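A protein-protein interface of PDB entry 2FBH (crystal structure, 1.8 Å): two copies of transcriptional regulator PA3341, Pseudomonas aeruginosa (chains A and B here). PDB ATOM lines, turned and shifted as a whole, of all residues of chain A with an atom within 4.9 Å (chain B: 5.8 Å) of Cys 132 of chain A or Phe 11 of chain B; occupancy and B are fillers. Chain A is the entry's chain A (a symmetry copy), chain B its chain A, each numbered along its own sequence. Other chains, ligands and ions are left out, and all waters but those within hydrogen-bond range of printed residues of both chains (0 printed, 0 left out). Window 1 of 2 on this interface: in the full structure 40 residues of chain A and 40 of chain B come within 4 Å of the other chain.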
ATOM      1  N   TRP A  22     -17.337 -21.022  37.177  1.00  0.00           N
ATOM      2  CA  TRP A  22     -17.124 -19.834  36.361  1.00  0.00           C
ATOM      3  C   TRP A  22     -16.922 -18.613  37.289  1.00  0.00           C
ATOM      4  O   TRP A  22     -15.967 -17.829  37.132  1.00  0.00           O
ATOM      5  CB  TRP A  22     -18.348 -19.638  35.472  1.00  0.00           C
ATOM      6  CG  TRP A  22     -18.269 -18.589  34.461  1.00  0.00           C
ATOM      7  CD1 TRP A  22     -17.631 -17.383  34.538  1.00  0.00           C
ATOM      8  CD2 TRP A  22     -18.951 -18.615  33.233  1.00  0.00           C
ATOM      9  NE1 TRP A  22     -17.873 -16.621  33.396  1.00  0.00           N
ATOM     10  CE2 TRP A  22     -18.670 -17.381  32.572  1.00  0.00           C
ATOM     11  CE3 TRP A  22     -19.784 -19.566  32.621  1.00  0.00           C
ATOM     12  CZ2 TRP A  22     -19.135 -17.081  31.309  1.00  0.00           C
ATOM     13  CZ3 TRP A  22     -20.297 -19.240  31.308  1.00  0.00           C
ATOM     14  CH2 TRP A  22     -19.970 -18.013  30.695  1.00  0.00           C
ATOM     15  N   ARG A 117     -15.165 -15.332  29.666  1.00  0.00           N
ATOM     16  CA  ARG A 117     -16.292 -15.800  28.765  1.00  0.00           C
ATOM     17  C   ARG A 117     -15.710 -16.409  27.513  1.00  0.00           C
ATOM     18  O   ARG A 117     -16.049 -17.557  27.172  1.00  0.00           O
ATOM     19  CB  ARG A 117     -17.233 -14.587  28.459  1.00  0.00           C
ATOM     20  CG  ARG A 117     -18.512 -14.996  27.738  1.00  0.00           C
ATOM     21  CD  ARG A 117     -19.357 -13.738  27.350  1.00  0.00           C
ATOM     22  NE  ARG A 117     -19.295 -12.775  28.384  1.00  0.00           N
ATOM     23  CZ  ARG A 117     -18.739 -11.558  28.381  1.00  0.00           C
ATOM     24  NH1 ARG A 117     -18.193 -10.949  27.336  1.00  0.00           N
ATOM     25  NH2 ARG A 117     -18.781 -10.910  29.487  1.00  0.00           N
ATOM     26  N   LEU A 121     -16.007 -20.611  26.866  1.00  0.00           N
ATOM     27  CA  LEU A 121     -16.825 -20.994  25.660  1.00  0.00           C
ATOM     28  C   LEU A 121     -15.991 -21.680  24.621  1.00  0.00           C
ATOM     29  O   LEU A 121     -16.515 -22.033  23.544  1.00  0.00           O
ATOM     30  CB  LEU A 121     -17.560 -19.796  25.089  1.00  0.00           C
ATOM     31  CG  LEU A 121     -18.601 -19.325  26.157  1.00  0.00           C
ATOM     32  CD1 LEU A 121     -19.254 -18.056  25.675  1.00  0.00           C
ATOM     33  CD2 LEU A 121     -19.646 -20.456  26.683  1.00  0.00           C
ATOM     34  N   GLU A 128     -25.084 -24.233  19.516  1.00  0.00           N
ATOM     35  CA  GLU A 128     -25.296 -24.950  20.773  1.00  0.00           C
ATOM     36  C   GLU A 128     -25.338 -24.014  21.997  1.00  0.00           C
ATOM     37  O   GLU A 128     -26.157 -24.266  22.882  1.00  0.00           O
ATOM     38  CB  GLU A 128     -24.299 -26.097  20.944  1.00  0.00           C
ATOM     39  CG  GLU A 128     -24.528 -27.135  19.862  1.00  0.00           C
ATOM     40  CD  GLU A 128     -23.618 -28.331  19.974  1.00  0.00           C
ATOM     41  OE1 GLU A 128     -22.724 -28.342  20.861  1.00  0.00           O
ATOM     42  OE2 GLU A 128     -23.896 -29.317  19.211  1.00  0.00           O
ATOM     43  N   GLN A 129     -24.512 -22.965  21.996  1.00  0.00           N
ATOM     44  CA  GLN A 129     -24.604 -21.921  22.992  1.00  0.00           C
ATOM     45  C   GLN A 129     -26.050 -21.360  23.002  1.00  0.00           C
ATOM     46  O   GLN A 129     -26.610 -21.129  24.056  1.00  0.00           O
ATOM     47  CB  GLN A 129     -23.619 -20.806  22.709  1.00  0.00           C
ATOM     48  CG  GLN A 129     -23.653 -19.778  23.842  1.00  0.00           C
ATOM     49  CD  GLN A 129     -22.685 -18.651  23.617  1.00  0.00           C
ATOM     50  OE1 GLN A 129     -21.647 -18.818  22.901  1.00  0.00           O
ATOM     51  NE2 GLN A 129     -22.960 -17.497  24.291  1.00  0.00           N
ATOM     52  N   ALA A 130     -26.536 -21.014  21.816  1.00  0.00           N
ATOM     53  CA  ALA A 130     -27.882 -20.437  21.718  1.00  0.00           C
ATOM     54  C   ALA A 130     -28.963 -21.357  22.256  1.00  0.00           C
ATOM     55  O   ALA A 130     -29.925 -20.899  22.956  1.00  0.00           O
ATOM     56  CB  ALA A 130     -28.104 -20.083  20.257  1.00  0.00           C
ATOM     57  N   LEU A 131     -28.839 -22.650  21.936  1.00  0.00           N
ATOM     58  CA  LEU A 131     -29.765 -23.646  22.407  1.00  0.00           C
ATOM     59  C   LEU A 131     -29.670 -23.736  23.929  1.00  0.00           C
ATOM     60  O   LEU A 131     -30.694 -23.776  24.627  1.00  0.00           O
ATOM     61  CB  LEU A 131     -29.457 -25.013  21.772  1.00  0.00           C
ATOM     62  CG  LEU A 131     -30.481 -26.110  22.128  1.00  0.00           C
ATOM     63  CD1 LEU A 131     -31.998 -25.604  22.080  1.00  0.00           C
ATOM     64  CD2 LEU A 131     -30.208 -27.356  21.331  1.00  0.00           C
ATOM     65  N   CYS A 132     -28.433 -23.775  24.445  1.00  0.00           N
ATOM     66  CA  CYS A 132     -28.206 -23.855  25.915  1.00  0.00           C
ATOM     67  C   CYS A 132     -28.914 -22.661  26.592  1.00  0.00           C
ATOM     68  O   CYS A 132     -29.600 -22.814  27.557  1.00  0.00           O
ATOM     69  CB  CYS A 132     -26.688 -23.785  26.181  1.00  0.00           C
ATOM     70  SG  CYS A 132     -26.279 -23.647  27.936  1.00  0.00           S
ATOM     71  N   GLN A 133     -28.747 -21.460  26.054  1.00  0.00           N
ATOM     72  CA  GLN A 133     -29.408 -20.292  26.588  1.00  0.00           C
ATOM     73  C   GLN A 133     -30.898 -20.390  26.569  1.00  0.00           C
ATOM     74  O   GLN A 133     -31.526 -20.017  27.574  1.00  0.00           O
ATOM     75  CB  GLN A 133     -28.965 -19.061  25.846  1.00  0.00           C
ATOM     76  CG  GLN A 133     -27.493 -18.755  26.149  1.00  0.00           C
ATOM     77  CD  GLN A 133     -26.977 -17.713  25.067  1.00  0.00           C
ATOM     78  OE1 GLN A 133     -27.567 -17.569  23.992  1.00  0.00           O
ATOM     79  NE2 GLN A 133     -25.899 -17.061  25.353  1.00  0.00           N
ATOM     80  N   GLN A 134     -31.484 -20.931  25.495  1.00  0.00           N
ATOM     81  CA  GLN A 134     -32.965 -21.086  25.449  1.00  0.00           C
ATOM     82  C   GLN A 134     -33.438 -22.076  26.538  1.00  0.00           C
ATOM     83  O   GLN A 134     -34.463 -21.842  27.185  1.00  0.00           O
ATOM     84  CB  GLN A 134     -33.471 -21.649  24.102  1.00  0.00           C
ATOM     85  CG  GLN A 134     -33.567 -20.691  22.989  1.00  0.00           C
ATOM     86  CD  GLN A 134     -34.293 -19.460  23.383  1.00  0.00           C
ATOM     87  OE1 GLN A 134     -35.469 -19.478  23.826  1.00  0.00           O
ATOM     88  NE2 GLN A 134     -33.649 -18.401  23.207  1.00  0.00           N
ATOM     89  N   VAL A 135     -32.724 -23.172  26.757  1.00  0.00           N
ATOM     90  CA  VAL A 135     -33.079 -24.104  27.864  1.00  0.00           C
ATOM     91  C   VAL A 135     -33.039 -23.381  29.201  1.00  0.00           C
ATOM     92  O   VAL A 135     -33.980 -23.449  29.977  1.00  0.00           O
ATOM     93  CB  VAL A 135     -32.169 -25.350  27.892  1.00  0.00           C
ATOM     94  CG1 VAL A 135     -32.501 -26.214  29.144  1.00  0.00           C
ATOM     95  CG2 VAL A 135     -32.512 -26.179  26.569  1.00  0.00           C
ATOM     96  N   LEU A 136     -31.912 -22.702  29.495  1.00  0.00           N
ATOM     97  CA  LEU A 136     -31.815 -21.924  30.752  1.00  0.00           C
ATOM     98  C   LEU A 136     -32.928 -20.864  30.905  1.00  0.00           C
ATOM     99  O   LEU A 136     -33.476 -20.712  31.997  1.00  0.00           O
ATOM    100  CB  LEU A 136     -30.463 -21.173  30.810  1.00  0.00           C
ATOM    101  CG  LEU A 136     -29.297 -22.180  30.921  1.00  0.00           C
ATOM    102  CD1 LEU A 136     -27.952 -21.404  30.879  1.00  0.00           C
ATOM    103  CD2 LEU A 136     -29.288 -23.188  32.042  1.00  0.00           C
ATOM    104  N   TYR B  10     -24.571 -12.044  28.201  1.00  0.00           N
ATOM    105  CA  TYR B  10     -23.816 -12.277  29.431  1.00  0.00           C
ATOM    106  C   TYR B  10     -24.298 -13.676  29.823  1.00  0.00           C
ATOM    107  O   TYR B  10     -25.164 -13.894  30.687  1.00  0.00           O
ATOM    108  CB  TYR B  10     -24.157 -11.238  30.427  1.00  0.00           C
ATOM    109  CG  TYR B  10     -23.766  -9.855  29.931  1.00  0.00           C
ATOM    110  CD1 TYR B  10     -24.692  -8.835  29.903  1.00  0.00           C
ATOM    111  CD2 TYR B  10     -22.428  -9.601  29.536  1.00  0.00           C
ATOM    112  CE1 TYR B  10     -24.304  -7.531  29.504  1.00  0.00           C
ATOM    113  CE2 TYR B  10     -22.023  -8.316  29.121  1.00  0.00           C
ATOM    114  CZ  TYR B  10     -22.966  -7.297  29.120  1.00  0.00           C
ATOM    115  OH  TYR B  10     -22.568  -6.026  28.731  1.00  0.00           O
ATOM    116  N   PHE B  11     -23.689 -14.615  29.107  1.00  0.00           N
ATOM    117  CA  PHE B  11     -23.996 -16.003  29.268  1.00  0.00           C
ATOM    118  C   PHE B  11     -23.745 -16.430  30.714  1.00  0.00           C
ATOM    119  O   PHE B  11     -24.532 -17.231  31.269  1.00  0.00           O
ATOM    120  CB  PHE B  11     -23.011 -16.758  28.367  1.00  0.00           C
ATOM    121  CG  PHE B  11     -23.289 -18.226  28.279  1.00  0.00           C
ATOM    122  CD1 PHE B  11     -23.822 -18.774  27.131  1.00  0.00           C
ATOM    123  CD2 PHE B  11     -22.963 -19.070  29.306  1.00  0.00           C
ATOM    124  CE1 PHE B  11     -24.050 -20.142  27.051  1.00  0.00           C
ATOM    125  CE2 PHE B  11     -23.220 -20.432  29.230  1.00  0.00           C
ATOM    126  CZ  PHE B  11     -23.773 -20.944  28.107  1.00  0.00           C
ATOM    127  N   GLY B  12     -22.631 -15.978  31.319  1.00  0.00           N
ATOM    128  CA  GLY B  12     -22.321 -16.435  32.669  1.00  0.00           C
ATOM    129  C   GLY B  12     -23.396 -15.937  33.657  1.00  0.00           C
ATOM    130  O   GLY B  12     -23.745 -16.643  34.602  1.00  0.00           O
ATOM    131  N   THR B  13     -23.900 -14.734  33.408  1.00  0.00           N
ATOM    132  CA  THR B  13     -24.915 -14.168  34.274  1.00  0.00           C
ATOM    133  C   THR B  13     -26.208 -14.938  34.163  1.00  0.00           C
ATOM    134  O   THR B  13     -26.847 -15.188  35.178  1.00  0.00           O
ATOM    135  CB  THR B  13     -25.182 -12.677  33.986  1.00  0.00           C
ATOM    136  OG1 THR B  13     -24.007 -11.958  34.359  1.00  0.00           O
ATOM    137  CG2 THR B  13     -26.293 -12.232  34.867  1.00  0.00           C
ATOM    138  N   LEU B  14     -26.577 -15.365  32.945  1.00  0.00           N
ATOM    139  CA  LEU B  14     -27.839 -16.148  32.774  1.00  0.00           C
ATOM    140  C   LEU B  14     -27.689 -17.487  33.535  1.00  0.00           C
ATOM    141  O   LEU B  14     -28.581 -17.919  34.296  1.00  0.00           O
ATOM    142  CB  LEU B  14     -28.107 -16.417  31.303  1.00  0.00           C
ATOM    143  CG  LEU B  14     -29.303 -17.386  31.087  1.00  0.00           C
ATOM    144  CD1 LEU B  14     -30.655 -16.834  31.558  1.00  0.00           C
ATOM    145  CD2 LEU B  14     -29.280 -17.751  29.574  1.00  0.00           C
ATOM    146  N   LEU B  15     -26.506 -18.109  33.456  1.00  0.00           N
ATOM    147  CA  LEU B  15     -26.295 -19.355  34.162  1.00  0.00           C
ATOM    148  C   LEU B  15     -26.399 -19.154  35.683  1.00  0.00           C
ATOM    149  O   LEU B  15     -27.048 -19.913  36.381  1.00  0.00           O
ATOM    150  CB  LEU B  15     -24.894 -19.921  33.772  1.00  0.00           C
ATOM    151  CG  LEU B  15     -24.338 -21.062  34.538  1.00  0.00           C
ATOM    152  CD1 LEU B  15     -25.323 -22.201  34.343  1.00  0.00           C
ATOM    153  CD2 LEU B  15     -22.995 -21.433  33.852  1.00  0.00           C
ATOM    154  N   ALA B  16     -25.784 -18.065  36.162  1.00  0.00           N
ATOM    155  CA  ALA B  16     -25.791 -17.853  37.638  1.00  0.00           C
ATOM    156  C   ALA B  16     -27.185 -17.564  38.134  1.00  0.00           C
ATOM    157  O   ALA B  16     -27.601 -17.998  39.255  1.00  0.00           O
ATOM    158  CB  ALA B  16     -24.886 -16.709  37.930  1.00  0.00           C
ATOM    159  N   CYS B 132     -28.077 -29.335  26.491  1.00  0.00           N
ATOM    160  CA  CYS B 132     -27.745 -28.301  27.511  1.00  0.00           C
ATOM    161  C   CYS B 132     -26.672 -28.873  28.464  1.00  0.00           C
ATOM    162  O   CYS B 132     -25.704 -28.239  28.758  1.00  0.00           O
ATOM    163  CB  CYS B 132     -29.026 -27.968  28.305  1.00  0.00           C
ATOM    164  SG  CYS B 132     -28.724 -26.892  29.724  1.00  0.00           S
ATOM    165  N   VAL B 135     -23.193 -28.928  26.820  1.00  0.00           N
ATOM    166  CA  VAL B 135     -22.586 -27.566  26.836  1.00  0.00           C
ATOM    167  C   VAL B 135     -22.019 -27.253  28.211  1.00  0.00           C
ATOM    168  O   VAL B 135     -20.876 -26.840  28.335  1.00  0.00           O
ATOM    169  CB  VAL B 135     -23.589 -26.477  26.400  1.00  0.00           C
ATOM    170  CG1 VAL B 135     -22.939 -25.072  26.563  1.00  0.00           C
ATOM    171  CG2 VAL B 135     -23.889 -26.745  24.852  1.00  0.00           C
ATOM    172  N   LEU B 136     -22.844 -27.417  29.265  1.00  0.00           N
ATOM    173  CA  LEU B 136     -22.350 -27.186  30.642  1.00  0.00           C
ATOM    174  C   LEU B 136     -21.121 -28.050  31.005  1.00  0.00           C
ATOM    175  O   LEU B 136     -20.188 -27.545  31.630  1.00  0.00           O
ATOM    176  CB  LEU B 136     -23.459 -27.524  31.668  1.00  0.00           C
ATOM    177  CG  LEU B 136     -24.630 -26.525  31.536  1.00  0.00           C
ATOM    178  CD1 LEU B 136     -25.766 -26.945  32.507  1.00  0.00           C
ATOM    179  CD2 LEU B 136     -24.362 -25.045  31.649  1.00  0.00           C
ATOM    180  N   ILE B 139     -18.069 -26.483  29.399  1.00  0.00           N
ATOM    181  CA  ILE B 139     -17.675 -25.257  30.152  1.00  0.00           C
ATOM    182  C   ILE B 139     -16.949 -25.685  31.406  1.00  0.00           C
ATOM    183  O   ILE B 139     -15.858 -25.193  31.759  1.00  0.00           O
ATOM    184  CB  ILE B 139     -18.950 -24.385  30.476  1.00  0.00           C
ATOM    185  CG1 ILE B 139     -19.557 -23.781  29.151  1.00  0.00           C
ATOM    186  CG2 ILE B 139     -18.571 -23.313  31.566  1.00  0.00           C
ATOM    187  CD1 ILE B 139     -20.964 -23.186  29.374  1.00  0.00           C
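The side-chain amide nitrogen (NE2) of Gln 129 of chain A sits close to the side-chain amide nitrogen (NE2) of Gln 133 of chain A, at 3.2 Å.
Among the printed residues, pairs that only touch across the chains: Gln 133 of chain A with Phe 11 of chain B (3.2 Å), Gln 129 of chain A with Phe 11 of chain B (3.2 Å), Trp 22 of chain A with Phe 11 of chain B (3.3 Å), Trp 22 of chain A with Gly 12 of chain B (3.4 Å), Cys 132 of chain A with Phe 11 of chain B (3.7 Å), Gln 133 of chain A with Leu 14 of chain B (3.8 Å), Leu 136 of chain A with Leu 14 of chain B (3.8 Å), Arg 117 of chain A with Tyr 10 of chain B (3.9 Å), Val 135 of chain A with Cys 132 of chain B (3.9 Å), Cys 132 of chain A with Val 135 of chain B (3.9 Å), Glu 128 of chain A with Val 135 of chain B (3.9 Å) and Trp 22 of chain A with Leu 15 of chain B (3.9 Å).
Printed residues of chain B within 4 Å of Trp 22 of chain A: Phe 11 (3.3 Å), Gly 12 (3.4 Å) and Leu 15 (3.9 Å). Of the printed residues of chain B, Glu 128 of chain A touches Val 135. Cys 132 of chain A touches two residues of chain B. Gln 134 of chain A touches none of the printed residues of chain B. Printed residues of chain A within 4 Å of Tyr 10 of chain B: Arg 117. Of the printed residues of chain A, Leu 14 of chain B touches Gln 133 and Leu 136. Printed residues of chain A within 4 Å of Cys 132 of chain B: Val 135 (3.9 Å). The nearest residue of chain B that does not touch Cys 132 of chain A is Leu 136 of chain B (4.4 Å). The nearest printed residue of chain A that does not touch Cys 132 of chain B is Leu 136 of chain A (4.4 Å).
Along chain B the printed residues that touch a printed residue of chain A span positions 10 to 135. Along chain A the printed residues that touch a printed residue of chain B span positions 22 to 136.
Cys 132 of chain A touches Val 135 of chain B, and with the chains exchanged Val 135 of chain A touches Cys 132 of chain B. Positions printed for both chains: 132, 135 and 136. Of the 12 pairs that touch across the chains among the printed residues, 2 have their exchanged pair printed and touching as well.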
